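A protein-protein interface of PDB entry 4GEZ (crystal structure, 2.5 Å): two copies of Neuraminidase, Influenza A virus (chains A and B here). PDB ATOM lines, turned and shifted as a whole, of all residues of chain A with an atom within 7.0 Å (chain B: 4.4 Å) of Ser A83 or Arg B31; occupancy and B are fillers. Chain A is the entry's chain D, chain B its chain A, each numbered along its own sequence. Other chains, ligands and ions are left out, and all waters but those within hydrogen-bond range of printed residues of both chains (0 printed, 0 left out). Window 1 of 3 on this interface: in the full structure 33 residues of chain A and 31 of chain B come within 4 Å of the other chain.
No position is printed for both chains.
O of Pro A103 is in hydrogen-bond range of ND2 of Asn A122, at 3.0 Å. O of Asp B377 lies within hydrogen-bond range of NH2 of Arg B31, 3.3 Å away. OG of Ser A83 sits close to SD of Met A100, 3.8 Å away. The backbone NH (N) of Ala A64 lies within hydrogen-bond range of the backbone carbonyl oxygen (O) of Ser A83, 2.7 Å away. NH2 of Arg B31 lies within hydrogen-bond range of O of Trp B376, at 2.6 Å. NH1 of Arg B31 is in salt-bridge range of OE1 of Glu B360 (3.7 Å).
Leu A45 touches none of the printed residues of chain B. Glu A82 touches none of the printed residues of chain B. Of chain B, only Arg B31 and Gly B32 come within 4 Å of Ser A83. Printed residues of chain B within 4 Å of Leu A102: Thr B29. Of the printed residues of chain A, Thr B29 touches Ile A101 and Leu A102. Arg B31 touches just these residues of chain A: Glu A81, Ser A83, Met A100 and Pro A103. Printed residues of chain A within 4 Å of Lys B321: Glu A81. The nearest printed residue of chain B that does not touch Ser A83 is His B30 (6.2 Å). The nearest residue of chain A that does not touch Arg B31 is Glu A82 (4.6 Å).
Of the 20 printed residues of chain A, 7 touch a printed residue of chain B. Hydrophobic or aromatic side chains of chain B within 4 Å of the printed part of chain A: His B30 and Trp B376. Among the printed residues, Asp or Glu carboxylates within 4 Å of a Lys or Arg side-chain nitrogen of the other chain: Glu A81 with Arg B31 (2.4 Å) and Glu A81 with Lys B321 (3.3 Å).
Among the printed residues, pairs that only touch across the chains: Asn A122 with Trp B376 (3.0 Å), Leu A102 with Thr B29 (3.5 Å), Pro A103 with Arg B31 (3.7 Å), Met A100 with His B30 (3.8 Å), Glu A81 with Gly B32 (3.9 Å) and Ser A83 with Gly B32 (3.9 Å).
NH2 of Arg B31 lies within salt-bridge range of OE2 of Glu A81 (2.4 Å). The side-chain hydroxyl of Ser A83 lies within hydrogen-bond range of the backbone carbonyl oxygen of Arg B31 (2.8 Å). The side-chain sulfur (SD) of Met A100 sits at hydrogen-bond distance from the backbone NH (N) of Arg B31, at 3.4 Å. OE2 of Glu A81 lies within salt-bridge range of NZ of Lys B321, 3.3 Å away. O of Thr B29 lies close to O of Ile A101, at 3.2 Å. OE2 of Glu A81 sits close to O of Asp B377, at 3.2 Å.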
ATOM      1  N   ILE A  44       2.025  18.204  20.704  1.00  0.00           N
ATOM      2  CA  ILE A  44       2.304  17.407  19.526  1.00  0.00           C
ATOM      3  C   ILE A  44       1.022  16.762  19.017  1.00  0.00           C
ATOM      4  O   ILE A  44       0.303  16.115  19.776  1.00  0.00           O
ATOM      5  CB  ILE A  44       3.368  16.325  19.822  1.00  0.00           C
ATOM      6  CG1 ILE A  44       4.672  16.978  20.285  1.00  0.00           C
ATOM      7  CG2 ILE A  44       3.624  15.483  18.591  1.00  0.00           C
ATOM      8  CD1 ILE A  44       5.734  15.993  20.740  1.00  0.00           C
ATOM      9  N   LEU A  45       0.733  16.957  17.734  1.00  0.00           N
ATOM     10  CA  LEU A  45      -0.443  16.356  17.115  1.00  0.00           C
ATOM     11  C   LEU A  45      -0.126  14.914  16.733  1.00  0.00           C
ATOM     12  O   LEU A  45       0.960  14.630  16.229  1.00  0.00           O
ATOM     13  CB  LEU A  45      -0.880  17.164  15.887  1.00  0.00           C
ATOM     14  CG  LEU A  45      -1.128  18.655  16.123  1.00  0.00           C
ATOM     15  CD1 LEU A  45      -1.486  19.372  14.832  1.00  0.00           C
ATOM     16  CD2 LEU A  45      -2.212  18.857  17.165  1.00  0.00           C
ATOM     17  N   PHE A  62       2.964   7.049  19.703  1.00  0.00           N
ATOM     18  CA  PHE A  62       2.143   7.704  18.692  1.00  0.00           C
ATOM     19  C   PHE A  62       2.943   8.164  17.489  1.00  0.00           C
ATOM     20  O   PHE A  62       4.164   8.313  17.560  1.00  0.00           O
ATOM     21  CB  PHE A  62       1.378   8.906  19.262  1.00  0.00           C
ATOM     22  CG  PHE A  62       2.243   9.935  19.957  1.00  0.00           C
ATOM     23  CD1 PHE A  62       2.792   9.691  21.211  1.00  0.00           C
ATOM     24  CD2 PHE A  62       2.514  11.149  19.338  1.00  0.00           C
ATOM     25  CE1 PHE A  62       3.570  10.652  21.842  1.00  0.00           C
ATOM     26  CE2 PHE A  62       3.290  12.110  19.954  1.00  0.00           C
ATOM     27  CZ  PHE A  62       3.821  11.864  21.208  1.00  0.00           C
ATOM     28  N   ILE A  63       2.231   8.402  16.391  1.00  0.00           N
ATOM     29  CA  ILE A  63       2.828   8.944  15.182  1.00  0.00           C
ATOM     30  C   ILE A  63       2.585  10.445  15.183  1.00  0.00           C
ATOM     31  O   ILE A  63       1.445  10.901  15.081  1.00  0.00           O
ATOM     32  CB  ILE A  63       2.220   8.302  13.912  1.00  0.00           C
ATOM     33  CG1 ILE A  63       2.376   6.777  13.962  1.00  0.00           C
ATOM     34  CG2 ILE A  63       2.837   8.896  12.651  1.00  0.00           C
ATOM     35  CD1 ILE A  63       3.823   6.296  13.998  1.00  0.00           C
ATOM     36  N   ALA A  64       3.664  11.210  15.300  1.00  0.00           N
ATOM     37  CA  ALA A  64       3.575  12.660  15.402  1.00  0.00           C
ATOM     38  C   ALA A  64       3.630  13.255  14.006  1.00  0.00           C
ATOM     39  O   ALA A  64       4.417  12.800  13.171  1.00  0.00           O
ATOM     40  CB  ALA A  64       4.707  13.190  16.249  1.00  0.00           C
ATOM     41  N   TYR A  65       2.809  14.273  13.752  1.00  0.00           N
ATOM     42  CA  TYR A  65       2.751  14.881  12.424  1.00  0.00           C
ATOM     43  C   TYR A  65       2.739  16.414  12.440  1.00  0.00           C
ATOM     44  O   TYR A  65       2.822  17.050  11.384  1.00  0.00           O
ATOM     45  CB  TYR A  65       1.557  14.336  11.625  1.00  0.00           C
ATOM     46  CG  TYR A  65       0.189  14.741  12.135  1.00  0.00           C
ATOM     47  CD1 TYR A  65      -0.375  15.960  11.776  1.00  0.00           C
ATOM     48  CD2 TYR A  65      -0.548  13.890  12.946  1.00  0.00           C
ATOM     49  CE1 TYR A  65      -1.620  16.327  12.229  1.00  0.00           C
ATOM     50  CE2 TYR A  65      -1.796  14.247  13.399  1.00  0.00           C
ATOM     51  CZ  TYR A  65      -2.325  15.468  13.036  1.00  0.00           C
ATOM     52  OH  TYR A  65      -3.569  15.838  13.485  1.00  0.00           O
ATOM     53  N   TRP A  80       2.466  13.127   5.540  1.00  0.00           N
ATOM     54  CA  TRP A  80       3.822  13.503   5.175  1.00  0.00           C
ATOM     55  C   TRP A  80       4.902  12.932   6.072  1.00  0.00           C
ATOM     56  O   TRP A  80       4.906  11.738   6.368  1.00  0.00           O
ATOM     57  CB  TRP A  80       3.950  15.028   5.113  1.00  0.00           C
ATOM     58  CG  TRP A  80       3.140  15.612   4.009  1.00  0.00           C
ATOM     59  CD1 TRP A  80       2.191  16.589   4.112  1.00  0.00           C
ATOM     60  CD2 TRP A  80       3.113  15.172   2.647  1.00  0.00           C
ATOM     61  NE1 TRP A  80       1.623  16.828   2.884  1.00  0.00           N
ATOM     62  CE2 TRP A  80       2.169  15.964   1.969  1.00  0.00           C
ATOM     63  CE3 TRP A  80       3.820  14.200   1.929  1.00  0.00           C
ATOM     64  CZ2 TRP A  80       1.910  15.813   0.609  1.00  0.00           C
ATOM     65  CZ3 TRP A  80       3.561  14.051   0.588  1.00  0.00           C
ATOM     66  CH2 TRP A  80       2.617  14.852  -0.062  1.00  0.00           C
ATOM     67  N   GLU A  81       5.815  13.787   6.516  1.00  0.00           N
ATOM     68  CA  GLU A  81       6.941  13.305   7.290  1.00  0.00           C
ATOM     69  C   GLU A  81       6.447  13.011   8.689  1.00  0.00           C
ATOM     70  O   GLU A  81       6.199  13.915   9.490  1.00  0.00           O
ATOM     71  CB  GLU A  81       8.068  14.339   7.307  1.00  0.00           C
ATOM     72  CG  GLU A  81       8.121  15.197   6.049  1.00  0.00           C
ATOM     73  CD  GLU A  81       9.172  16.287   6.113  1.00  0.00           C
ATOM     74  OE1 GLU A  81       8.886  17.366   6.675  1.00  0.00           O
ATOM     75  OE2 GLU A  81      10.294  16.056   5.622  1.00  0.00           O
ATOM     76  N   GLU A  82       6.307  11.723   8.974  1.00  0.00           N
ATOM     77  CA  GLU A  82       5.721  11.283  10.221  1.00  0.00           C
ATOM     78  C   GLU A  82       6.802  10.616  11.049  1.00  0.00           C
ATOM     79  O   GLU A  82       7.734  10.013  10.511  1.00  0.00           O
ATOM     80  CB  GLU A  82       4.559  10.319   9.954  1.00  0.00           C
ATOM     81  CG  GLU A  82       3.360  10.967   9.266  1.00  0.00           C
ATOM     82  CD  GLU A  82       2.255   9.978   8.928  1.00  0.00           C
ATOM     83  OE1 GLU A  82       1.078  10.266   9.244  1.00  0.00           O
ATOM     84  OE2 GLU A  82       2.559   8.925   8.332  1.00  0.00           O
ATOM     85  N   SER A  83       6.670  10.709  12.364  1.00  0.00           N
ATOM     86  CA  SER A  83       7.710  10.210  13.244  1.00  0.00           C
ATOM     87  C   SER A  83       7.088   9.604  14.487  1.00  0.00           C
ATOM     88  O   SER A  83       6.142  10.157  15.053  1.00  0.00           O
ATOM     89  CB  SER A  83       8.671  11.347  13.610  1.00  0.00           C
ATOM     90  OG  SER A  83       9.837  10.853  14.240  1.00  0.00           O
ATOM     91  N   LEU A  84       7.634   8.475  14.925  1.00  0.00           N
ATOM     92  CA  LEU A  84       7.112   7.797  16.106  1.00  0.00           C
ATOM     93  C   LEU A  84       7.702   8.409  17.374  1.00  0.00           C
ATOM     94  O   LEU A  84       8.924   8.558  17.497  1.00  0.00           O
ATOM     95  CB  LEU A  84       7.415   6.296  16.045  1.00  0.00           C
ATOM     96  CG  LEU A  84       7.023   5.488  17.280  1.00  0.00           C
ATOM     97  CD1 LEU A  84       5.508   5.330  17.360  1.00  0.00           C
ATOM     98  CD2 LEU A  84       7.713   4.133  17.308  1.00  0.00           C
ATOM     99  N   TYR A  85       6.825   8.757  18.313  1.00  0.00           N
ATOM    100  CA  TYR A  85       7.213   9.378  19.575  1.00  0.00           C
ATOM    101  C   TYR A  85       6.645   8.589  20.751  1.00  0.00           C
ATOM    102  O   TYR A  85       5.737   7.769  20.581  1.00  0.00           O
ATOM    103  CB  TYR A  85       6.669  10.804  19.644  1.00  0.00           C
ATOM    104  CG  TYR A  85       7.552  11.876  19.055  1.00  0.00           C
ATOM    105  CD1 TYR A  85       7.826  11.908  17.694  1.00  0.00           C
ATOM    106  CD2 TYR A  85       8.071  12.885  19.854  1.00  0.00           C
ATOM    107  CE1 TYR A  85       8.611  12.896  17.151  1.00  0.00           C
ATOM    108  CE2 TYR A  85       8.860  13.881  19.319  1.00  0.00           C
ATOM    109  CZ  TYR A  85       9.124  13.879  17.964  1.00  0.00           C
ATOM    110  OH  TYR A  85       9.908  14.865  17.409  1.00  0.00           O
ATOM    111  N   MET A 100      11.513  11.512  20.768  1.00  0.00           N
ATOM    112  CA  MET A 100      11.518  10.874  19.453  1.00  0.00           C
ATOM    113  C   MET A 100      12.148   9.491  19.551  1.00  0.00           C
ATOM    114  O   MET A 100      13.126   9.297  20.274  1.00  0.00           O
ATOM    115  CB  MET A 100      12.275  11.707  18.414  1.00  0.00           C
ATOM    116  CG  MET A 100      12.031  11.221  16.986  1.00  0.00           C
ATOM    117  SD  MET A 100      13.169  11.867  15.747  1.00  0.00           S
ATOM    118  CE  MET A 100      13.307  13.590  16.230  1.00  0.00           C
ATOM    119  N   ILE A 101      11.567   8.534  18.836  1.00  0.00           N
ATOM    120  CA  ILE A 101      12.097   7.177  18.765  1.00  0.00           C
ATOM    121  C   ILE A 101      12.633   6.894  17.358  1.00  0.00           C
ATOM    122  O   ILE A 101      13.837   6.726  17.173  1.00  0.00           O
ATOM    123  CB  ILE A 101      11.022   6.126  19.137  1.00  0.00           C
ATOM    124  CG1 ILE A 101      10.423   6.432  20.511  1.00  0.00           C
ATOM    125  CG2 ILE A 101      11.610   4.722  19.136  1.00  0.00           C
ATOM    126  CD1 ILE A 101       9.323   5.477  20.930  1.00  0.00           C
ATOM    127  N   LEU A 102      11.738   6.866  16.371  1.00  0.00           N
ATOM    128  CA  LEU A 102      12.115   6.609  14.983  1.00  0.00           C
ATOM    129  C   LEU A 102      11.144   7.282  14.014  1.00  0.00           C
ATOM    130  O   LEU A 102       9.981   7.519  14.353  1.00  0.00           O
ATOM    131  CB  LEU A 102      12.120   5.097  14.706  1.00  0.00           C
ATOM    132  CG  LEU A 102      13.281   4.247  15.229  1.00  0.00           C
ATOM    133  CD1 LEU A 102      13.075   2.765  14.940  1.00  0.00           C
ATOM    134  CD2 LEU A 102      14.595   4.718  14.635  1.00  0.00           C
ATOM    135  N   PRO A 103      11.615   7.590  12.795  1.00  0.00           N
ATOM    136  CA  PRO A 103      10.664   7.999  11.758  1.00  0.00           C
ATOM    137  C   PRO A 103       9.773   6.806  11.445  1.00  0.00           C
ATOM    138  O   PRO A 103      10.268   5.678  11.461  1.00  0.00           O
ATOM    139  CB  PRO A 103      11.566   8.322  10.558  1.00  0.00           C
ATOM    140  CG  PRO A 103      12.842   7.576  10.814  1.00  0.00           C
ATOM    141  CD  PRO A 103      13.006   7.572  12.306  1.00  0.00           C
ATOM    142  N   GLY A 104       8.491   7.031  11.176  1.00  0.00           N
ATOM    143  CA  GLY A 104       7.584   5.917  10.964  1.00  0.00           C
ATOM    144  C   GLY A 104       6.182   6.333  10.556  1.00  0.00           C
ATOM    145  O   GLY A 104       5.732   7.445  10.846  1.00  0.00           O
ATOM    146  N   ARG A 105       5.487   5.413   9.894  1.00  0.00           N
ATOM    147  CA  ARG A 105       4.162   5.662   9.350  1.00  0.00           C
ATOM    148  C   ARG A 105       3.171   4.809  10.138  1.00  0.00           C
ATOM    149  O   ARG A 105       2.013   5.189  10.352  1.00  0.00           O
ATOM    150  CB  ARG A 105       4.177   5.287   7.866  1.00  0.00           C
ATOM    151  CG  ARG A 105       3.376   6.195   6.952  1.00  0.00           C
ATOM    152  CD  ARG A 105       4.182   6.512   5.697  1.00  0.00           C
ATOM    153  NE  ARG A 105       5.236   7.479   5.995  1.00  0.00           N
ATOM    154  CZ  ARG A 105       5.066   8.798   5.980  1.00  0.00           C
ATOM    155  NH1 ARG A 105       3.884   9.312   5.671  1.00  0.00           N
ATOM    156  NH2 ARG A 105       6.079   9.602   6.272  1.00  0.00           N
ATOM    157  N   VAL A 120       9.087   0.098  13.281  1.00  0.00           N
ATOM    158  CA  VAL A 120       8.431   1.110  12.464  1.00  0.00           C
ATOM    159  C   VAL A 120       8.459   0.665  11.011  1.00  0.00           C
ATOM    160  O   VAL A 120       9.376  -0.034  10.583  1.00  0.00           O
ATOM    161  CB  VAL A 120       9.090   2.503  12.595  1.00  0.00           C
ATOM    162  CG1 VAL A 120       8.886   3.062  13.992  1.00  0.00           C
ATOM    163  CG2 VAL A 120      10.568   2.433  12.248  1.00  0.00           C
ATOM    164  N   ASN A 122       8.230   2.171   7.044  1.00  0.00           N
ATOM    165  CA  ASN A 122       8.316   3.409   6.283  1.00  0.00           C
ATOM    166  C   ASN A 122       8.155   3.169   4.798  1.00  0.00           C
ATOM    167  O   ASN A 122       8.460   2.086   4.302  1.00  0.00           O
ATOM    168  CB  ASN A 122       9.644   4.122   6.530  1.00  0.00           C
ATOM    169  CG  ASN A 122       9.704   4.799   7.883  1.00  0.00           C
ATOM    170  OD1 ASN A 122       9.566   6.018   7.980  1.00  0.00           O
ATOM    171  ND2 ASN A 122       9.966   4.024   8.927  1.00  0.00           N
ATOM    172  N   THR B  29      17.777   7.077  12.229  1.00  0.00           N
ATOM    173  CA  THR B  29      17.454   6.824  13.622  1.00  0.00           C
ATOM    174  C   THR B  29      16.707   8.031  14.174  1.00  0.00           C
ATOM    175  O   THR B  29      15.928   7.916  15.116  1.00  0.00           O
ATOM    176  CB  THR B  29      18.723   6.541  14.462  1.00  0.00           C
ATOM    177  OG1 THR B  29      19.725   7.531  14.188  1.00  0.00           O
ATOM    178  CG2 THR B  29      19.277   5.167  14.130  1.00  0.00           C
ATOM    179  N   HIS B  30      16.929   9.184  13.553  1.00  0.00           N
ATOM    180  CA  HIS B  30      16.204  10.394  13.917  1.00  0.00           C
ATOM    181  C   HIS B  30      15.802  11.205  12.696  1.00  0.00           C
ATOM    182  O   HIS B  30      16.632  11.593  11.874  1.00  0.00           O
ATOM    183  CB  HIS B  30      17.013  11.243  14.897  1.00  0.00           C
ATOM    184  CG  HIS B  30      17.193  10.598  16.232  1.00  0.00           C
ATOM    185  ND1 HIS B  30      18.246   9.765  16.530  1.00  0.00           N
ATOM    186  CD2 HIS B  30      16.426  10.655  17.353  1.00  0.00           C
ATOM    187  CE1 HIS B  30      18.128   9.340  17.776  1.00  0.00           C
ATOM    188  NE2 HIS B  30      17.037   9.862  18.295  1.00  0.00           N
ATOM    189  N   ARG B  31      14.501  11.451  12.610  1.00  0.00           N
ATOM    190  CA  ARG B  31      13.890  12.158  11.504  1.00  0.00           C
ATOM    191  C   ARG B  31      12.507  12.536  12.006  1.00  0.00           C
ATOM    192  O   ARG B  31      11.671  11.661  12.252  1.00  0.00           O
ATOM    193  CB  ARG B  31      13.797  11.238  10.285  1.00  0.00           C
ATOM    194  CG  ARG B  31      12.943  11.760   9.149  1.00  0.00           C
ATOM    195  CD  ARG B  31      13.607  12.947   8.501  1.00  0.00           C
ATOM    196  NE  ARG B  31      13.131  13.169   7.141  1.00  0.00           N
ATOM    197  CZ  ARG B  31      12.326  14.166   6.796  1.00  0.00           C
ATOM    198  NH1 ARG B  31      11.898  15.016   7.720  1.00  0.00           N
ATOM    199  NH2 ARG B  31      11.940  14.306   5.536  1.00  0.00           N
ATOM    200  N   GLY B  32      12.267  13.837  12.153  1.00  0.00           N
ATOM    201  CA  GLY B  32      11.071  14.318  12.820  1.00  0.00           C
ATOM    202  C   GLY B  32       9.952  14.708  11.877  1.00  0.00           C
ATOM    203  O   GLY B  32       9.894  14.240  10.741  1.00  0.00           O
ATOM    204  N   PHE B 318      17.904  11.642  -0.048  1.00  0.00           N
ATOM    205  CA  PHE B 318      17.062  12.808  -0.261  1.00  0.00           C
ATOM    206  C   PHE B 318      17.210  13.292  -1.698  1.00  0.00           C
ATOM    207  O   PHE B 318      18.272  13.138  -2.303  1.00  0.00           O
ATOM    208  CB  PHE B 318      17.461  13.932   0.704  1.00  0.00           C
ATOM    209  CG  PHE B 318      17.194  13.622   2.149  1.00  0.00           C
ATOM    210  CD1 PHE B 318      15.947  13.877   2.707  1.00  0.00           C
ATOM    211  CD2 PHE B 318      18.194  13.095   2.957  1.00  0.00           C
ATOM    212  CE1 PHE B 318      15.693  13.599   4.045  1.00  0.00           C
ATOM    213  CE2 PHE B 318      17.952  12.816   4.297  1.00  0.00           C
ATOM    214  CZ  PHE B 318      16.697  13.070   4.843  1.00  0.00           C
ATOM    215  N   LYS B 321      14.917  17.706  -0.585  1.00  0.00           N
ATOM    216  CA  LYS B 321      15.246  18.286   0.709  1.00  0.00           C
ATOM    217  C   LYS B 321      16.507  19.127   0.649  1.00  0.00           C
ATOM    218  O   LYS B 321      17.528  18.687   0.117  1.00  0.00           O
ATOM    219  CB  LYS B 321      15.421  17.175   1.749  1.00  0.00           C
ATOM    220  CG  LYS B 321      14.166  16.870   2.542  1.00  0.00           C
ATOM    221  CD  LYS B 321      14.168  17.640   3.847  1.00  0.00           C
ATOM    222  CE  LYS B 321      12.893  17.402   4.630  1.00  0.00           C
ATOM    223  NZ  LYS B 321      12.914  18.087   5.953  1.00  0.00           N
ATOM    224  N   ILE B 348      18.992  18.830   7.868  1.00  0.00           N
ATOM    225  CA  ILE B 348      17.954  18.915   6.849  1.00  0.00           C
ATOM    226  C   ILE B 348      16.990  20.041   7.183  1.00  0.00           C
ATOM    227  O   ILE B 348      16.509  20.148   8.318  1.00  0.00           O
ATOM    228  CB  ILE B 348      17.184  17.586   6.668  1.00  0.00           C
ATOM    229  CG1 ILE B 348      16.667  17.061   8.003  1.00  0.00           C
ATOM    230  CG2 ILE B 348      18.064  16.551   5.969  1.00  0.00           C
ATOM    231  CD1 ILE B 348      15.756  15.844   7.870  1.00  0.00           C
ATOM    232  N   GLU B 360      16.659  20.682  10.939  1.00  0.00           N
ATOM    233  CA  GLU B 360      16.538  19.472  11.734  1.00  0.00           C
ATOM    234  C   GLU B 360      17.855  18.709  11.666  1.00  0.00           C
ATOM    235  O   GLU B 360      18.460  18.583  10.593  1.00  0.00           O
ATOM    236  CB  GLU B 360      15.382  18.600  11.243  1.00  0.00           C
ATOM    237  CG  GLU B 360      15.110  17.399  12.139  1.00  0.00           C
ATOM    238  CD  GLU B 360      14.218  16.367  11.490  1.00  0.00           C
ATOM    239  OE1 GLU B 360      13.483  16.711  10.540  1.00  0.00           O
ATOM    240  OE2 GLU B 360      14.260  15.203  11.935  1.00  0.00           O
ATOM    241  N   TRP B 376      13.659   9.790   1.687  1.00  0.00           N
ATOM    242  CA  TRP B 376      13.158  10.285   2.968  1.00  0.00           C
ATOM    243  C   TRP B 376      12.577  11.704   2.929  1.00  0.00           C
ATOM    244  O   TRP B 376      12.413  12.339   3.973  1.00  0.00           O
ATOM    245  CB  TRP B 376      14.243  10.156   4.043  1.00  0.00           C
ATOM    246  CG  TRP B 376      14.565   8.721   4.331  1.00  0.00           C
ATOM    247  CD1 TRP B 376      15.641   8.004   3.886  1.00  0.00           C
ATOM    248  CD2 TRP B 376      13.775   7.817   5.107  1.00  0.00           C
ATOM    249  NE1 TRP B 376      15.571   6.712   4.351  1.00  0.00           N
ATOM    250  CE2 TRP B 376      14.431   6.571   5.102  1.00  0.00           C
ATOM    251  CE3 TRP B 376      12.576   7.942   5.812  1.00  0.00           C
ATOM    252  CZ2 TRP B 376      13.924   5.457   5.775  1.00  0.00           C
ATOM    253  CZ3 TRP B 376      12.079   6.845   6.481  1.00  0.00           C
ATOM    254  CH2 TRP B 376      12.752   5.620   6.463  1.00  0.00           C
ATOM    255  N   ASP B 377      12.280  12.202   1.731  1.00  0.00           N
ATOM    256  CA  ASP B 377      11.567  13.470   1.582  1.00  0.00           C
ATOM    257  C   ASP B 377      10.178  13.379   2.214  1.00  0.00           C
ATOM    258  O   ASP B 377       9.785  14.229   3.016  1.00  0.00           O
ATOM    259  CB  ASP B 377      11.429  13.852   0.105  1.00  0.00           C
ATOM    260  CG  ASP B 377      12.748  14.265  -0.522  1.00  0.00           C
ATOM    261  OD1 ASP B 377      13.717  14.512   0.230  1.00  0.00           O
ATOM    262  OD2 ASP B 377      12.816  14.345  -1.768  1.00  0.00           O
